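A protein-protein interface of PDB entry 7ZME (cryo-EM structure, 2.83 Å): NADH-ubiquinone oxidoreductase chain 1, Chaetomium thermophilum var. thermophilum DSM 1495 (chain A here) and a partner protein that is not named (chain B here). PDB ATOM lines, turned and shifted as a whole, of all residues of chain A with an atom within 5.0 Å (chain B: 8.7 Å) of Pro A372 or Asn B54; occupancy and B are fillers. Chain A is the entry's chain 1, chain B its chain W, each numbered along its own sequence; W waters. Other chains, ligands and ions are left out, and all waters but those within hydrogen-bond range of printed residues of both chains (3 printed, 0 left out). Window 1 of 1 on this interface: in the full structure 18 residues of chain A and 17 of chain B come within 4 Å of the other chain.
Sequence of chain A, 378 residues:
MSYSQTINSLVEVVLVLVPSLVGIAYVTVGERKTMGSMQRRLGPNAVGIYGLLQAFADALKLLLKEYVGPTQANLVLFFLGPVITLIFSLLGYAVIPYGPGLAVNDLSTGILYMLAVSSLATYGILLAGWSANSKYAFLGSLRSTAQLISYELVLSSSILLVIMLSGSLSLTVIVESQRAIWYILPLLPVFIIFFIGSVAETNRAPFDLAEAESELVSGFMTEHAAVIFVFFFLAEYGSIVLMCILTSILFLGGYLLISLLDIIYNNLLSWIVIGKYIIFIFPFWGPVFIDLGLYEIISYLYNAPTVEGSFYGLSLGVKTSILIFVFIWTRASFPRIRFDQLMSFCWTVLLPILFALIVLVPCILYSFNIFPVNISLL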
ATOM      1  N   MET A 164      -6.198   5.822  16.525  1.00  0.00           N
ATOM      2  CA  MET A 164      -5.795   4.406  16.362  1.00  0.00           C
ATOM      3  C   MET A 164      -4.713   4.066  17.389  1.00  0.00           C
ATOM      4  O   MET A 164      -4.525   2.884  17.661  1.00  0.00           O
ATOM      5  CB  MET A 164      -5.284   4.145  14.949  1.00  0.00           C
ATOM      6  CG  MET A 164      -6.374   4.030  13.909  1.00  0.00           C
ATOM      7  SD  MET A 164      -5.694   3.915  12.236  1.00  0.00           S
ATOM      8  CE  MET A 164      -7.189   3.636  11.292  1.00  0.00           C
ATOM      9  N   LEU A 165      -4.032   5.072  17.941  1.00  0.00           N
ATOM     10  CA  LEU A 165      -3.013   4.829  18.995  1.00  0.00           C
ATOM     11  C   LEU A 165      -3.618   5.021  20.385  1.00  0.00           C
ATOM     12  O   LEU A 165      -3.310   4.208  21.243  1.00  0.00           O
ATOM     13  CB  LEU A 165      -1.834   5.789  18.815  1.00  0.00           C
ATOM     14  CG  LEU A 165      -1.061   5.729  17.503  1.00  0.00           C
ATOM     15  CD1 LEU A 165       0.247   6.486  17.653  1.00  0.00           C
ATOM     16  CD2 LEU A 165      -0.785   4.293  17.102  1.00  0.00           C
ATOM     17  N   SER A 166      -4.422   6.062  20.601  1.00  0.00           N
ATOM     18  CA  SER A 166      -4.991   6.365  21.943  1.00  0.00           C
ATOM     19  C   SER A 166      -6.179   5.448  22.234  1.00  0.00           C
ATOM     20  O   SER A 166      -6.322   5.045  23.392  1.00  0.00           O
ATOM     21  CB  SER A 166      -5.381   7.810  22.027  1.00  0.00           C
ATOM     22  OG  SER A 166      -6.350   8.132  21.044  1.00  0.00           O
ATOM     23  N   GLY A 167      -6.997   5.155  21.217  1.00  0.00           N
ATOM     24  CA  GLY A 167      -8.184   4.293  21.356  1.00  0.00           C
ATOM     25  C   GLY A 167      -9.310   4.976  22.092  1.00  0.00           C
ATOM     26  O   GLY A 167     -10.221   4.262  22.531  1.00  0.00           O
ATOM     27  N   ASN A 369       1.509  -6.438  18.702  1.00  0.00           N
ATOM     28  CA  ASN A 369       0.553  -6.626  19.830  1.00  0.00           C
ATOM     29  C   ASN A 369       0.316  -5.300  20.542  1.00  0.00           C
ATOM     30  O   ASN A 369       0.215  -5.308  21.773  1.00  0.00           O
ATOM     31  CB  ASN A 369       0.971  -7.722  20.813  1.00  0.00           C
ATOM     32  CG  ASN A 369      -0.195  -8.316  21.569  1.00  0.00           C
ATOM     33  OD1 ASN A 369      -0.054  -8.703  22.724  1.00  0.00           O
ATOM     34  ND2 ASN A 369      -1.351  -8.377  20.931  1.00  0.00           N
ATOM     35  N   ILE A 370       0.260  -4.204  19.785  1.00  0.00           N
ATOM     36  CA  ILE A 370       0.140  -2.867  20.431  1.00  0.00           C
ATOM     37  C   ILE A 370      -1.209  -2.198  20.184  1.00  0.00           C
ATOM     38  O   ILE A 370      -1.227  -0.969  20.110  1.00  0.00           O
ATOM     39  CB  ILE A 370       1.375  -1.959  20.228  1.00  0.00           C
ATOM     40  CG1 ILE A 370       1.819  -1.858  18.769  1.00  0.00           C
ATOM     41  CG2 ILE A 370       2.510  -2.418  21.128  1.00  0.00           C
ATOM     42  CD1 ILE A 370       2.749  -0.703  18.508  1.00  0.00           C
ATOM     43  N   PHE A 371      -2.293  -2.958  20.034  1.00  0.00           N
ATOM     44  CA  PHE A 371      -3.636  -2.319  19.943  1.00  0.00           C
ATOM     45  C   PHE A 371      -4.018  -1.860  21.354  1.00  0.00           C
ATOM     46  O   PHE A 371      -3.997  -2.670  22.286  1.00  0.00           O
ATOM     47  CB  PHE A 371      -4.714  -3.251  19.381  1.00  0.00           C
ATOM     48  CG  PHE A 371      -4.787  -3.368  17.880  1.00  0.00           C
ATOM     49  CD1 PHE A 371      -4.496  -2.290  17.062  1.00  0.00           C
ATOM     50  CD2 PHE A 371      -5.189  -4.552  17.285  1.00  0.00           C
ATOM     51  CE1 PHE A 371      -4.587  -2.399  15.684  1.00  0.00           C
ATOM     52  CE2 PHE A 371      -5.279  -4.660  15.907  1.00  0.00           C
ATOM     53  CZ  PHE A 371      -4.977  -3.585  15.108  1.00  0.00           C
ATOM     54  N   PRO A 372      -4.345  -0.568  21.550  1.00  0.00           N
ATOM     55  CA  PRO A 372      -4.752  -0.071  22.859  1.00  0.00           C
ATOM     56  C   PRO A 372      -6.096  -0.627  23.357  1.00  0.00           C
ATOM     57  O   PRO A 372      -6.986  -0.819  22.563  1.00  0.00           O
ATOM     58  CB  PRO A 372      -4.822   1.445  22.622  1.00  0.00           C
ATOM     59  CG  PRO A 372      -5.143   1.577  21.158  1.00  0.00           C
ATOM     60  CD  PRO A 372      -4.341   0.468  20.516  1.00  0.00           C
ATOM     61  N   VAL A 373      -6.186  -0.903  24.656  1.00  0.00           N
ATOM     62  CA  VAL A 373      -7.481  -1.332  25.258  1.00  0.00           C
ATOM     63  C   VAL A 373      -8.446  -0.158  25.105  1.00  0.00           C
ATOM     64  O   VAL A 373      -8.016   0.985  25.309  1.00  0.00           O
ATOM     65  CB  VAL A 373      -7.348  -1.848  26.704  1.00  0.00           C
ATOM     66  CG1 VAL A 373      -6.763  -3.246  26.756  1.00  0.00           C
ATOM     67  CG2 VAL A 373      -6.543  -0.901  27.576  1.00  0.00           C
ATOM     68  N   ASN A 374      -9.698  -0.420  24.749  1.00  0.00           N
ATOM     69  CA  ASN A 374     -10.641   0.678  24.419  1.00  0.00           C
ATOM     70  C   ASN A 374     -11.563   0.888  25.612  1.00  0.00           C
ATOM     71  O   ASN A 374     -12.629   1.484  25.445  1.00  0.00           O
ATOM     72  CB  ASN A 374     -11.231   0.473  23.026  1.00  0.00           C
ATOM     73  CG  ASN A 374     -10.160   0.366  21.964  1.00  0.00           C
ATOM     74  OD1 ASN A 374      -9.646   1.368  21.486  1.00  0.00           O
ATOM     75  ND2 ASN A 374      -9.808  -0.851  21.598  1.00  0.00           N
ATOM     76  N   LEU B  46       6.498   3.681  22.024  1.00  0.00           N
ATOM     77  CA  LEU B  46       5.070   3.409  21.941  1.00  0.00           C
ATOM     78  C   LEU B  46       4.777   1.929  22.151  1.00  0.00           C
ATOM     79  O   LEU B  46       3.750   1.575  22.738  1.00  0.00           O
ATOM     80  CB  LEU B  46       4.531   3.883  20.594  1.00  0.00           C
ATOM     81  CG  LEU B  46       3.016   4.050  20.512  1.00  0.00           C
ATOM     82  CD1 LEU B  46       2.587   5.410  21.044  1.00  0.00           C
ATOM     83  CD2 LEU B  46       2.541   3.846  19.091  1.00  0.00           C
ATOM     84  N   VAL B  47       5.641   1.047  21.646  1.00  0.00           N
ATOM     85  CA  VAL B  47       5.464  -0.410  21.906  1.00  0.00           C
ATOM     86  C   VAL B  47       5.439  -0.625  23.421  1.00  0.00           C
ATOM     87  O   VAL B  47       4.451  -1.170  23.912  1.00  0.00           O
ATOM     88  CB  VAL B  47       6.496  -1.297  21.179  1.00  0.00           C
ATOM     89  CG1 VAL B  47       6.569  -2.693  21.770  1.00  0.00           C
ATOM     90  CG2 VAL B  47       6.227  -1.368  19.685  1.00  0.00           C
ATOM     91  N   LYS B  48       6.458  -0.132  24.126  1.00  0.00           N
ATOM     92  CA  LYS B  48       6.579  -0.317  25.591  1.00  0.00           C
ATOM     93  C   LYS B  48       5.400   0.311  26.327  1.00  0.00           C
ATOM     94  O   LYS B  48       4.903  -0.333  27.257  1.00  0.00           O
ATOM     95  CB  LYS B  48       7.861   0.384  26.052  1.00  0.00           C
ATOM     96  CG  LYS B  48       9.155  -0.125  25.432  1.00  0.00           C
ATOM     97  CD  LYS B  48       9.569  -1.473  25.970  1.00  0.00           C
ATOM     98  CE  LYS B  48       9.703  -1.478  27.478  1.00  0.00           C
ATOM     99  NZ  LYS B  48       9.831  -2.853  28.016  1.00  0.00           N
ATOM    100  N   GLY B  49       4.970   1.509  25.923  1.00  0.00           N
ATOM    101  CA  GLY B  49       3.867   2.210  26.602  1.00  0.00           C
ATOM    102  C   GLY B  49       2.569   1.445  26.549  1.00  0.00           C
ATOM    103  O   GLY B  49       1.929   1.301  27.597  1.00  0.00           O
ATOM    104  N   ILE B  50       2.155   1.058  25.342  1.00  0.00           N
ATOM    105  CA  ILE B  50       0.860   0.348  25.146  1.00  0.00           C
ATOM    106  C   ILE B  50       0.927  -1.030  25.797  1.00  0.00           C
ATOM    107  O   ILE B  50      -0.075  -1.458  26.370  1.00  0.00           O
ATOM    108  CB  ILE B  50       0.456   0.304  23.658  1.00  0.00           C
ATOM    109  CG1 ILE B  50       0.497   1.697  23.025  1.00  0.00           C
ATOM    110  CG2 ILE B  50      -0.902  -0.352  23.473  1.00  0.00           C
ATOM    111  CD1 ILE B  50       0.161   1.714  21.555  1.00  0.00           C
ATOM    112  N   ARG B  51       2.075  -1.691  25.708  1.00  0.00           N
ATOM    113  CA  ARG B  51       2.217  -3.010  26.362  1.00  0.00           C
ATOM    114  C   ARG B  51       2.019  -2.835  27.870  1.00  0.00           C
ATOM    115  O   ARG B  51       1.293  -3.653  28.452  1.00  0.00           O
ATOM    116  CB  ARG B  51       3.520  -3.673  25.912  1.00  0.00           C
ATOM    117  CG  ARG B  51       3.432  -4.292  24.527  1.00  0.00           C
ATOM    118  CD  ARG B  51       4.641  -5.135  24.193  1.00  0.00           C
ATOM    119  NE  ARG B  51       4.674  -5.598  22.815  1.00  0.00           N
ATOM    120  CZ  ARG B  51       5.696  -6.251  22.278  1.00  0.00           C
ATOM    121  NH1 ARG B  51       5.654  -6.630  21.013  1.00  0.00           N
ATOM    122  NH2 ARG B  51       6.762  -6.517  23.009  1.00  0.00           N
ATOM    123  N   GLU B  52       2.590  -1.782  28.462  1.00  0.00           N
ATOM    124  CA  GLU B  52       2.422  -1.487  29.911  1.00  0.00           C
ATOM    125  C   GLU B  52       0.970  -1.139  30.232  1.00  0.00           C
ATOM    126  O   GLU B  52       0.493  -1.587  31.276  1.00  0.00           O
ATOM    127  CB  GLU B  52       3.374  -0.362  30.318  1.00  0.00           C
ATOM    128  CG  GLU B  52       3.264   0.048  31.772  1.00  0.00           C
ATOM    129  CD  GLU B  52       4.584   0.029  32.520  1.00  0.00           C
ATOM    130  OE1 GLU B  52       5.544  -0.563  31.997  1.00  0.00           O
ATOM    131  OE2 GLU B  52       4.650   0.610  33.617  1.00  0.00           O
ATOM    132  N   GLN B  53       0.318  -0.333  29.387  1.00  0.00           N
ATOM    133  CA  GLN B  53      -1.087   0.095  29.625  1.00  0.00           C
ATOM    134  C   GLN B  53      -2.057  -1.088  29.516  1.00  0.00           C
ATOM    135  O   GLN B  53      -3.006  -1.125  30.296  1.00  0.00           O
ATOM    136  CB  GLN B  53      -1.460   1.325  28.799  1.00  0.00           C
ATOM    137  CG  GLN B  53      -1.981   1.016  27.408  1.00  0.00           C
ATOM    138  CD  GLN B  53      -2.339   2.272  26.658  1.00  0.00           C
ATOM    139  OE1 GLN B  53      -2.043   3.383  27.091  1.00  0.00           O
ATOM    140  NE2 GLN B  53      -2.986   2.099  25.520  1.00  0.00           N
ATOM    141  N   ASN B  54      -1.833  -2.001  28.576  1.00  0.00           N
ATOM    142  CA  ASN B  54      -2.710  -3.184  28.422  1.00  0.00           C
ATOM    143  C   ASN B  54      -2.563  -4.034  29.678  1.00  0.00           C
ATOM    144  O   ASN B  54      -3.547  -4.684  30.050  1.00  0.00           O
ATOM    145  CB  ASN B  54      -2.478  -3.909  27.091  1.00  0.00           C
ATOM    146  CG  ASN B  54      -2.951  -3.118  25.891  1.00  0.00           C
ATOM    147  OD1 ASN B  54      -3.504  -2.030  26.033  1.00  0.00           O
ATOM    148  ND2 ASN B  54      -2.741  -3.655  24.703  1.00  0.00           N
ATOM    149  N   GLU B  55      -1.376  -4.037  30.290  1.00  0.00           N
ATOM    150  CA  GLU B  55      -1.157  -4.747  31.577  1.00  0.00           C
ATOM    151  C   GLU B  55      -1.823  -4.007  32.743  1.00  0.00           C
ATOM    152  O   GLU B  55      -2.371  -4.686  33.620  1.00  0.00           O
ATOM    153  CB  GLU B  55       0.331  -5.035  31.743  1.00  0.00           C
ATOM    154  CG  GLU B  55       0.831  -6.069  30.758  1.00  0.00           C
ATOM    155  CD  GLU B  55      -0.116  -7.245  30.598  1.00  0.00           C
ATOM    156  OE1 GLU B  55      -0.530  -7.522  29.455  1.00  0.00           O
ATOM    157  OE2 GLU B  55      -0.431  -7.888  31.618  1.00  0.00           O
ATOM    158  N   LEU B  56      -1.766  -2.678  32.768  1.00  0.00           N
ATOM    159  CA  LEU B  56      -2.452  -1.864  33.805  1.00  0.00           C
ATOM    160  C   LEU B  56      -3.956  -2.093  33.682  1.00  0.00           C
ATOM    161  O   LEU B  56      -4.633  -2.090  34.720  1.00  0.00           O
ATOM    162  CB  LEU B  56      -2.120  -0.392  33.554  1.00  0.00           C
ATOM    163  CG  LEU B  56      -0.702   0.051  33.903  1.00  0.00           C
ATOM    164  CD1 LEU B  56      -0.529   1.530  33.610  1.00  0.00           C
ATOM    165  CD2 LEU B  56      -0.396  -0.236  35.359  1.00  0.00           C
ATOM    166  N   ALA B  57      -4.451  -2.226  32.451  1.00  0.00           N
ATOM    167  CA  ALA B  57      -5.882  -2.506  32.199  1.00  0.00           C
ATOM    168  C   ALA B  57      -6.268  -3.867  32.779  1.00  0.00           C
ATOM    169  O   ALA B  57      -7.390  -3.984  33.281  1.00  0.00           O
ATOM    170  CB  ALA B  57      -6.161  -2.414  30.727  1.00  0.00           C
ATOM    171  N   ARG B  58      -5.376  -4.858  32.693  1.00  0.00           N
ATOM    172  CA  ARG B  58      -5.635  -6.208  33.262  1.00  0.00           C
ATOM    173  C   ARG B  58      -5.776  -6.120  34.782  1.00  0.00           C
ATOM    174  O   ARG B  58      -6.654  -6.797  35.325  1.00  0.00           O
ATOM    175  CB  ARG B  58      -4.499  -7.155  32.877  1.00  0.00           C
ATOM    176  CG  ARG B  58      -4.710  -8.599  33.307  1.00  0.00           C
ATOM    177  CD  ARG B  58      -3.478  -9.451  33.080  1.00  0.00           C
ATOM    178  NE  ARG B  58      -2.891  -9.219  31.771  1.00  0.00           N
ATOM    179  CZ  ARG B  58      -3.250  -9.841  30.656  1.00  0.00           C
ATOM    180  NH1 ARG B  58      -2.646  -9.547  29.520  1.00  0.00           N
ATOM    181  NH2 ARG B  58      -4.209 -10.749  30.676  1.00  0.00           N
ATOM    182  N   GLU B  59      -4.965  -5.289  35.433  1.00  0.00           N
ATOM    183  CA  GLU B  59      -4.992  -5.142  36.910  1.00  0.00           C
ATOM    184  C   GLU B  59      -6.285  -4.450  37.335  1.00  0.00           C
ATOM    185  O   GLU B  59      -6.883  -4.900  38.320  1.00  0.00           O
ATOM    186  CB  GLU B  59      -3.698  -4.474  37.359  1.00  0.00           C
ATOM    187  CG  GLU B  59      -3.615  -4.197  38.845  1.00  0.00           C
ATOM    188  CD  GLU B  59      -2.403  -3.356  39.193  1.00  0.00           C
ATOM    189  OE1 GLU B  59      -1.669  -2.987  38.265  1.00  0.00           O
ATOM    190  OE2 GLU B  59      -2.203  -3.062  40.379  1.00  0.00           O
ATOM    191  N   LYS B  60      -6.698  -3.406  36.613  1.00  0.00           N
ATOM    192  CA  LYS B  60      -7.953  -2.657  36.916  1.00  0.00           C
ATOM    193  C   LYS B  60      -9.159  -3.581  36.765  1.00  0.00           C
ATOM    194  O   LYS B  60     -10.128  -3.391  37.500  1.00  0.00           O
ATOM    195  CB  LYS B  60      -8.115  -1.471  35.965  1.00  0.00           C
ATOM    196  CG  LYS B  60      -9.304  -0.567  36.247  1.00  0.00           C
ATOM    197  CD  LYS B  60      -9.347   0.654  35.368  1.00  0.00           C
ATOM    198  CE  LYS B  60     -10.386   1.652  35.820  1.00  0.00           C
ATOM    199  NZ  LYS B  60     -10.202   2.961  35.156  1.00  0.00           N
ATOM    200  N   MET B  61      -9.084  -4.557  35.863  1.00  0.00           N
ATOM    201  CA  MET B  61     -10.252  -5.421  35.589  1.00  0.00           C
ATOM    202  C   MET B  61     -10.325  -6.544  36.621  1.00  0.00           C
ATOM    203  O   MET B  61     -11.440  -6.830  37.049  1.00  0.00           O
ATOM    204  CB  MET B  61     -10.210  -5.992  34.169  1.00  0.00           C
ATOM    205  CG  MET B  61     -10.478  -4.970  33.076  1.00  0.00           C
ATOM    206  SD  MET B  61     -12.116  -4.198  33.142  1.00  0.00           S
ATOM    207  CE  MET B  61     -11.727  -2.598  33.846  1.00  0.00           C
HETATM  208  O   HOH W   1      -2.460   4.070  23.591  1.00  0.00           O
HETATM  209  O   HOH W   2       0.008  -5.731  24.505  1.00  0.00           O
HETATM  210  O   HOH W   3      -5.491   2.160  26.890  1.00  0.00           O
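The side-chain amide nitrogen of Asn B54 sits at hydrogen-bond distance from the backbone carbonyl oxygen of Phe A371, 2.9 Å away.
The side-chain amide oxygen (OD1) of Asn B54 sits at hydrogen-bond distance from the backbone NH (N) of Val A373, at 3.2 Å.
Of the printed residues of chain B, Leu A165 touches Leu B46 (3.8 Å).
Of the printed residues of chain B, Phe A371 touches Asn B54.
Of chain B, only Ile B50 (3.9 Å), Gln B53 (3.5 Å) and Asn B54 (3.9 Å) come within 4 Å of Pro A372.
Lys B48 touches none of the printed residues of chain A.
Of the printed residues of chain A, Arg B51 touches Ile A370.
Of the printed residues of chain A, Gln B53 touches Pro A372.
Asn B54 touches three residues of chain A.
Of the printed residues of chain A, Ala B57 touches Val A373 (3.5 Å).
The nearest residue of chain A that does not touch Asn B54 is Asn A369 (4.5 Å).
The nearest printed residue of chain A that does not touch Ile B50 is Phe A371 (4.04 Å).
Leu A165 touches Leu B46.
Val B47 touches Ile A370.
Ile A370 touches Ile B50.
CG2 of Ile A370 touches CG of Arg B51, at 3.99 Å.
Pro A372 touches Ile B50 (CA to CG2, 3.9 Å).
Gln B53 touches Pro A372 (NE2 to CB, 3.5 Å).
Pro A372 touches Asn B54 (CA to OD1, 3.9 Å).
Ala B57 touches Val A373.
Water W1 bridges the backbone carbonyl oxygen (O) of Leu A165 (2.5 Å) and the side-chain amide nitrogen (NE2) of Gln B53 (2.8 Å).
Water W2 bridges O of Asn A369 (2.8 Å) and ND2 of Asn B54 (3.5 Å).
Water W3 lies within hydrogen-bond range of NE2 of Gln B53 (2.9 Å) and O of Val A373 (3.2 Å).
Of the 10 printed residues of chain A, 5 touch a printed residue of chain B.
Hydrophobic or aromatic side chains of chain A that line the printed part of chain B: Leu A165, Ile A370, Pro A372 and Val A373.
Of the 16 printed residues of chain B, 7 touch a printed residue of chain A.
Among the printed residues, 10 pairs touch across the chains.
The backbone carbonyl oxygen of Pro A372 lies within hydrogen-bond range of the side-chain amide nitrogen of Asn A374 (3.0 Å).
O of Ile B50 sits close to OD1 of Asn B54 (3.5 Å).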
